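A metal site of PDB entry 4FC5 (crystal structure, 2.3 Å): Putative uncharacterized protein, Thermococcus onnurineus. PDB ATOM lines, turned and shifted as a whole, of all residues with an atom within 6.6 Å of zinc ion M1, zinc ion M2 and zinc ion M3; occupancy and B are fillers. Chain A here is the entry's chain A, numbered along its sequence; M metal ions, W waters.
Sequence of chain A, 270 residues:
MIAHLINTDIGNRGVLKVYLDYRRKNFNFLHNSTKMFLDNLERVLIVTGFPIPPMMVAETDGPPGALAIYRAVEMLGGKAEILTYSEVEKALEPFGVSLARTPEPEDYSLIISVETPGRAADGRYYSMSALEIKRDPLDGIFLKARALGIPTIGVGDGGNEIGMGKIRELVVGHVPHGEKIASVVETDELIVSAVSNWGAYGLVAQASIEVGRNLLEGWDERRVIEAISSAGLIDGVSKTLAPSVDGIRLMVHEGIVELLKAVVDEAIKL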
ATOM      1  N   PHE A  50      16.212  -6.897  22.534  1.00  0.00           N
ATOM      2  CA  PHE A  50      16.317  -8.324  22.284  1.00  0.00           C
ATOM      3  C   PHE A  50      15.700  -8.702  20.943  1.00  0.00           C
ATOM      4  O   PHE A  50      14.485  -8.772  20.799  1.00  0.00           O
ATOM      5  CB  PHE A  50      15.638  -9.126  23.400  1.00  0.00           C
ATOM      6  CG  PHE A  50      16.252 -10.459  23.633  1.00  0.00           C
ATOM      7  CD1 PHE A  50      17.138 -10.646  24.690  1.00  0.00           C
ATOM      8  CD2 PHE A  50      15.993 -11.517  22.776  1.00  0.00           C
ATOM      9  CE1 PHE A  50      17.750 -11.870  24.890  1.00  0.00           C
ATOM     10  CE2 PHE A  50      16.607 -12.755  22.972  1.00  0.00           C
ATOM     11  CZ  PHE A  50      17.480 -12.930  24.033  1.00  0.00           C
ATOM     12  N   ILE A  52      14.187 -10.722  17.961  1.00  0.00           N
ATOM     13  CA  ILE A  52      13.405 -11.946  17.964  1.00  0.00           C
ATOM     14  C   ILE A  52      13.362 -12.623  16.605  1.00  0.00           C
ATOM     15  O   ILE A  52      12.875 -12.043  15.642  1.00  0.00           O
ATOM     16  CB  ILE A  52      11.996 -11.629  18.472  1.00  0.00           C
ATOM     17  CG1 ILE A  52      12.096 -11.262  19.940  1.00  0.00           C
ATOM     18  CG2 ILE A  52      11.047 -12.809  18.257  1.00  0.00           C
ATOM     19  CD1 ILE A  52      10.832 -10.894  20.571  1.00  0.00           C
ATOM     20  N   GLU A  59      11.978  -6.541  20.957  1.00  0.00           N
ATOM     21  CA  GLU A  59      10.679  -6.730  21.555  1.00  0.00           C
ATOM     22  C   GLU A  59      10.369  -5.672  22.584  1.00  0.00           C
ATOM     23  O   GLU A  59      11.217  -4.832  22.874  1.00  0.00           O
ATOM     24  CB  GLU A  59      10.598  -8.127  22.196  1.00  0.00           C
ATOM     25  CG  GLU A  59      11.609  -8.368  23.293  1.00  0.00           C
ATOM     26  CD  GLU A  59      11.373  -9.649  24.064  1.00  0.00           C
ATOM     27  OE1 GLU A  59      12.138 -10.614  23.863  1.00  0.00           O
ATOM     28  OE2 GLU A  59      10.425  -9.691  24.878  1.00  0.00           O
ATOM     29  N   THR A  60       9.153  -5.729  23.133  1.00  0.00           N
ATOM     30  CA  THR A  60       8.683  -4.783  24.149  1.00  0.00           C
ATOM     31  C   THR A  60       9.164  -5.054  25.585  1.00  0.00           C
ATOM     32  O   THR A  60       8.953  -4.233  26.475  1.00  0.00           O
ATOM     33  CB  THR A  60       7.146  -4.722  24.146  1.00  0.00           C
ATOM     34  OG1 THR A  60       6.619  -6.015  23.847  1.00  0.00           O
ATOM     35  CG2 THR A  60       6.649  -3.721  23.112  1.00  0.00           C
ATOM     36  N   ASP A  61       9.779  -6.199  25.823  1.00  0.00           N
ATOM     37  CA  ASP A  61      10.307  -6.457  27.155  1.00  0.00           C
ATOM     38  C   ASP A  61      11.713  -5.907  27.126  1.00  0.00           C
ATOM     39  O   ASP A  61      12.484  -6.238  26.205  1.00  0.00           O
ATOM     40  CB  ASP A  61      10.383  -7.945  27.452  1.00  0.00           C
ATOM     41  CG  ASP A  61      10.653  -8.233  28.899  1.00  0.00           C
ATOM     42  OD1 ASP A  61      10.998  -9.394  29.222  1.00  0.00           O
ATOM     43  OD2 ASP A  61      10.524  -7.318  29.737  1.00  0.00           O
ATOM     44  N   GLY A  62      12.054  -5.076  28.107  1.00  0.00           N
ATOM     45  CA  GLY A  62      13.381  -4.486  28.163  1.00  0.00           C
ATOM     46  C   GLY A  62      13.394  -2.971  28.052  1.00  0.00           C
ATOM     47  O   GLY A  62      13.754  -2.279  29.005  1.00  0.00           O
ATOM     48  N   GLU A 115      17.170  -7.174  29.689  1.00  0.00           N
ATOM     49  CA  GLU A 115      16.776  -8.009  28.548  1.00  0.00           C
ATOM     50  C   GLU A 115      17.653  -7.761  27.328  1.00  0.00           C
ATOM     51  O   GLU A 115      17.253  -7.061  26.402  1.00  0.00           O
ATOM     52  CB  GLU A 115      15.306  -7.762  28.172  1.00  0.00           C
ATOM     53  CG  GLU A 115      14.678  -8.910  27.384  1.00  0.00           C
ATOM     54  CD  GLU A 115      14.638 -10.200  28.167  1.00  0.00           C
ATOM     55  OE1 GLU A 115      15.110 -10.208  29.319  1.00  0.00           O
ATOM     56  OE2 GLU A 115      14.128 -11.205  27.643  1.00  0.00           O
ATOM     57  N   MET A 128      14.452 -17.832  23.315  1.00  0.00           N
ATOM     58  CA  MET A 128      13.898 -18.859  24.197  1.00  0.00           C
ATOM     59  C   MET A 128      13.586 -20.141  23.439  1.00  0.00           C
ATOM     60  O   MET A 128      13.539 -21.220  24.034  1.00  0.00           O
ATOM     61  CB  MET A 128      12.648 -18.353  24.927  1.00  0.00           C
ATOM     62  CG  MET A 128      12.918 -17.326  26.026  1.00  0.00           C
ATOM     63  SD  MET A 128      14.337 -17.709  27.098  1.00  0.00           S
ATOM     64  CE  MET A 128      13.715 -19.027  28.135  1.00  0.00           C
ATOM     65  N   GLY A 156      17.224 -10.276  33.722  1.00  0.00           N
ATOM     66  CA  GLY A 156      16.686 -11.239  32.769  1.00  0.00           C
ATOM     67  C   GLY A 156      15.552 -12.061  33.368  1.00  0.00           C
ATOM     68  O   GLY A 156      15.322 -12.034  34.573  1.00  0.00           O
ATOM     69  N   ASP A 157      14.872 -12.824  32.524  1.00  0.00           N
ATOM     70  CA  ASP A 157      13.743 -13.633  32.970  1.00  0.00           C
ATOM     71  C   ASP A 157      13.701 -14.980  32.282  1.00  0.00           C
ATOM     72  O   ASP A 157      12.698 -15.686  32.371  1.00  0.00           O
ATOM     73  CB  ASP A 157      12.434 -12.888  32.659  1.00  0.00           C
ATOM     74  CG  ASP A 157      12.325 -12.493  31.194  1.00  0.00           C
ATOM     75  OD1 ASP A 157      13.319 -12.660  30.447  1.00  0.00           O
ATOM     76  OD2 ASP A 157      11.252 -12.002  30.787  1.00  0.00           O
ATOM     77  N   GLY A 158      14.780 -15.347  31.600  1.00  0.00           N
ATOM     78  CA  GLY A 158      14.793 -16.614  30.909  1.00  0.00           C
ATOM     79  C   GLY A 158      16.079 -17.418  30.944  1.00  0.00           C
ATOM     80  O   GLY A 158      16.033 -18.640  30.969  1.00  0.00           O
ATOM     81  N   GLY A 159      17.225 -16.749  30.921  1.00  0.00           N
ATOM     82  CA  GLY A 159      18.468 -17.494  30.978  1.00  0.00           C
ATOM     83  C   GLY A 159      19.413 -17.271  29.812  1.00  0.00           C
ATOM     84  O   GLY A 159      20.527 -17.798  29.790  1.00  0.00           O
ATOM     85  N   ASN A 160      18.988 -16.505  28.827  1.00  0.00           N
ATOM     86  CA  ASN A 160      19.836 -16.257  27.706  1.00  0.00           C
ATOM     87  C   ASN A 160      20.172 -14.764  27.636  1.00  0.00           C
ATOM     88  O   ASN A 160      20.570 -14.267  26.606  1.00  0.00           O
ATOM     89  CB  ASN A 160      19.123 -16.709  26.440  1.00  0.00           C
ATOM     90  CG  ASN A 160      17.813 -16.000  26.237  1.00  0.00           C
ATOM     91  OD1 ASN A 160      17.257 -15.425  27.177  1.00  0.00           O
ATOM     92  ND2 ASN A 160      17.300 -16.039  25.014  1.00  0.00           N
ATOM     93  N   GLU A 161      19.991 -14.066  28.761  1.00  0.00           N
ATOM     94  CA  GLU A 161      20.270 -12.633  28.841  1.00  0.00           C
ATOM     95  C   GLU A 161      21.596 -12.325  29.515  1.00  0.00           C
ATOM     96  O   GLU A 161      22.069 -13.088  30.334  1.00  0.00           O
ATOM     97  CB  GLU A 161      19.148 -11.912  29.597  1.00  0.00           C
ATOM     98  CG  GLU A 161      17.764 -12.084  29.027  1.00  0.00           C
ATOM     99  CD  GLU A 161      17.036 -13.277  29.606  1.00  0.00           C
ATOM    100  OE1 GLU A 161      17.686 -14.284  29.980  1.00  0.00           O
ATOM    101  OE2 GLU A 161      15.788 -13.221  29.688  1.00  0.00           O
ATOM    102  N   MET A 164      23.025 -13.604  33.168  1.00  0.00           N
ATOM    103  CA  MET A 164      22.504 -14.926  33.506  1.00  0.00           C
ATOM    104  C   MET A 164      23.618 -15.978  33.517  1.00  0.00           C
ATOM    105  O   MET A 164      23.410 -17.132  33.887  1.00  0.00           O
ATOM    106  CB  MET A 164      21.433 -15.309  32.476  1.00  0.00           C
ATOM    107  CG  MET A 164      20.293 -16.155  33.008  1.00  0.00           C
ATOM    108  SD  MET A 164      19.156 -15.336  34.129  1.00  0.00           S
ATOM    109  CE  MET A 164      18.012 -14.611  33.020  1.00  0.00           C
ATOM    110  N   ALA A 194       9.990 -12.624  36.550  1.00  0.00           N
ATOM    111  CA  ALA A 194       9.146 -13.256  35.522  1.00  0.00           C
ATOM    112  C   ALA A 194       9.187 -12.497  34.223  1.00  0.00           C
ATOM    113  O   ALA A 194       9.091 -13.089  33.153  1.00  0.00           O
ATOM    114  CB  ALA A 194       7.690 -13.344  36.008  1.00  0.00           C
ATOM    115  N   VAL A 195       9.318 -11.182  34.338  1.00  0.00           N
ATOM    116  CA  VAL A 195       9.383 -10.283  33.183  1.00  0.00           C
ATOM    117  C   VAL A 195      10.437  -9.252  33.507  1.00  0.00           C
ATOM    118  O   VAL A 195      10.313  -8.539  34.505  1.00  0.00           O
ATOM    119  CB  VAL A 195       8.037  -9.544  32.984  1.00  0.00           C
ATOM    120  CG1 VAL A 195       8.183  -8.493  31.906  1.00  0.00           C
ATOM    121  CG2 VAL A 195       6.946 -10.551  32.634  1.00  0.00           C
ATOM    122  N   SER A 196      11.463  -9.144  32.655  1.00  0.00           N
ATOM    123  CA  SER A 196      12.568  -8.214  32.900  1.00  0.00           C
ATOM    124  C   SER A 196      12.153  -6.809  33.280  1.00  0.00           C
ATOM    125  O   SER A 196      12.674  -6.247  34.246  1.00  0.00           O
ATOM    126  CB  SER A 196      13.513  -8.184  31.697  1.00  0.00           C
ATOM    127  OG  SER A 196      14.060  -9.476  31.452  1.00  0.00           O
ATOM    128  N   ASN A 197      11.210  -6.232  32.547  1.00  0.00           N
ATOM    129  CA  ASN A 197      10.754  -4.883  32.861  1.00  0.00           C
ATOM    130  C   ASN A 197      10.481  -4.778  34.361  1.00  0.00           C
ATOM    131  O   ASN A 197      10.916  -3.838  35.013  1.00  0.00           O
ATOM    132  CB  ASN A 197       9.482  -4.541  32.084  1.00  0.00           C
ATOM    133  CG  ASN A 197       9.727  -4.373  30.587  1.00  0.00           C
ATOM    134  OD1 ASN A 197       8.827  -4.578  29.775  1.00  0.00           O
ATOM    135  ND2 ASN A 197      10.939  -3.993  30.211  1.00  0.00           N
ATOM    136  N   ASP A 235       5.793  -8.033  20.408  1.00  0.00           N
ATOM    137  CA  ASP A 235       5.598  -8.846  21.586  1.00  0.00           C
ATOM    138  C   ASP A 235       6.477 -10.067  21.335  1.00  0.00           C
ATOM    139  O   ASP A 235       6.396 -10.683  20.279  1.00  0.00           O
ATOM    140  CB  ASP A 235       4.138  -9.279  21.707  1.00  0.00           C
ATOM    141  CG  ASP A 235       3.923 -10.247  22.838  1.00  0.00           C
ATOM    142  OD1 ASP A 235       3.696  -9.809  23.991  1.00  0.00           O
ATOM    143  OD2 ASP A 235       3.994 -11.467  22.557  1.00  0.00           O
ATOM    144  N   GLY A 236       7.322 -10.405  22.297  1.00  0.00           N
ATOM    145  CA  GLY A 236       8.223 -11.529  22.133  1.00  0.00           C
ATOM    146  C   GLY A 236       7.601 -12.895  21.954  1.00  0.00           C
ATOM    147  O   GLY A 236       8.205 -13.764  21.328  1.00  0.00           O
ATOM    148  N   VAL A 237       6.404 -13.090  22.496  1.00  0.00           N
ATOM    149  CA  VAL A 237       5.746 -14.380  22.387  1.00  0.00           C
ATOM    150  C   VAL A 237       4.849 -14.492  21.144  1.00  0.00           C
ATOM    151  O   VAL A 237       4.904 -15.481  20.416  1.00  0.00           O
ATOM    152  CB  VAL A 237       4.923 -14.685  23.652  1.00  0.00           C
ATOM    153  CG1 VAL A 237       3.962 -15.813  23.387  1.00  0.00           C
ATOM    154  CG2 VAL A 237       5.860 -15.060  24.788  1.00  0.00           C
ATOM    155  N   VAL A 245       3.691  -7.364  26.649  1.00  0.00           N
ATOM    156  CA  VAL A 245       5.080  -7.775  26.773  1.00  0.00           C
ATOM    157  C   VAL A 245       5.089  -9.223  27.236  1.00  0.00           C
ATOM    158  O   VAL A 245       4.413  -9.575  28.200  1.00  0.00           O
ATOM    159  CB  VAL A 245       5.856  -6.829  27.724  1.00  0.00           C
ATOM    160  CG1 VAL A 245       4.909  -6.060  28.585  1.00  0.00           C
ATOM    161  CG2 VAL A 245       6.823  -7.605  28.573  1.00  0.00           C
ATOM    162  N   ASP A 246       5.826 -10.053  26.523  1.00  0.00           N
ATOM    163  CA  ASP A 246       5.938 -11.469  26.809  1.00  0.00           C
ATOM    164  C   ASP A 246       4.579 -12.136  26.925  1.00  0.00           C
ATOM    165  O   ASP A 246       4.365 -12.981  27.790  1.00  0.00           O
ATOM    166  CB  ASP A 246       6.726 -11.704  28.096  1.00  0.00           C
ATOM    167  CG  ASP A 246       8.156 -11.223  27.993  1.00  0.00           C
ATOM    168  OD1 ASP A 246       8.657 -11.076  26.869  1.00  0.00           O
ATOM    169  OD2 ASP A 246       8.782 -11.008  29.045  1.00  0.00           O
HETATM  170 ZN    ZN M   1      10.939 -11.169  28.819  1.00  0.00          ZN
HETATM  171 ZN    ZN M   2      14.235 -13.089  28.417  1.00  0.00          ZN
HETATM  172 ZN    ZN M   3      10.405 -11.495  25.791  1.00  0.00          ZN
HETATM  173  O   HOH W   1      14.906 -13.380  26.339  1.00  0.00           O
HETATM  174  O   HOH W   2       9.921 -13.707  24.942  1.00  0.00           O
HETATM  175  O   HOH W   3      11.880 -14.480  28.846  1.00  0.00           O
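The backbone NH (N) of Ser 196 lies close to the side-chain carboxylate (OD1) of Asp 61 (3.5 Å). OD2 of Asp 61 lies within hydrogen-bond range of N of Asn 197 (3.1 Å). The side-chain carboxylate of Glu 161 lies close to the side-chain amide oxygen of Asn 160, at 3.1 Å. The side-chain carboxylate of Glu 161 lies within hydrogen-bond range of the backbone NH of Gly 159. The backbone carbonyl oxygen (O) of Phe 50 lies within hydrogen-bond range of the backbone NH (N) of Glu 59 (3.4 Å). The side-chain carboxylate of Glu 115 sits at hydrogen-bond distance from the side-chain hydroxyl of Ser 196 (2.5 Å). N of Asp 246 is in hydrogen-bond range of OD1 of Asp 235 (3.3 Å). OD1 of Asp 157 lies close to OG of Ser 196, at 3.4 Å.
Of the 24 residues printed, 4 come within 4 Å of zinc ion M1.
Merely in contact with zinc ion M2: Gly 158 (3.9 Å). Four residues have an atom within 4 Å of zinc ion M2: Glu 115, Asp 157, Gly 158 and Glu 161.
Within 4 Å of zinc ion M3: Glu 59, Asp 61 and Asp 246.
OD1 of Asp 61 is bound to zinc ion M1 (1.8 Å). Zinc ion M1 is bound by OD2 of Asp 157, at 2.2 Å. The side-chain carboxylate (OD2) of Asp 246 is bound to zinc ion M1, at 2.2 Å. Zinc ion M1 has three donor atoms within binding distance.
Zinc ion M2 is bound by the side-chain carboxylate of Glu 161 (2.0 Å), the side-chain carboxylate of Glu 115 (2.0 Å), water W1 (2.2 Å) and the side-chain carboxylate of Asp 157 (2.3 Å). Zinc ion M2 has four donor atoms within binding distance. Slightly farther from zinc ion M2 lies water W3 (2.8 Å).
OE2 of Glu 59 is bound to zinc ion M3, 2.0 Å away. Zinc ion M3 is bound by the side-chain carboxylate (OD1) of Asp 246. Zinc ion M3 is bound by water W2, 2.4 Å away. Zinc ion M3 has three donor atoms within binding distance. Slightly farther from zinc ion M3 lies the side-chain carboxylate (OE1) of Glu 59 (2.7 Å).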
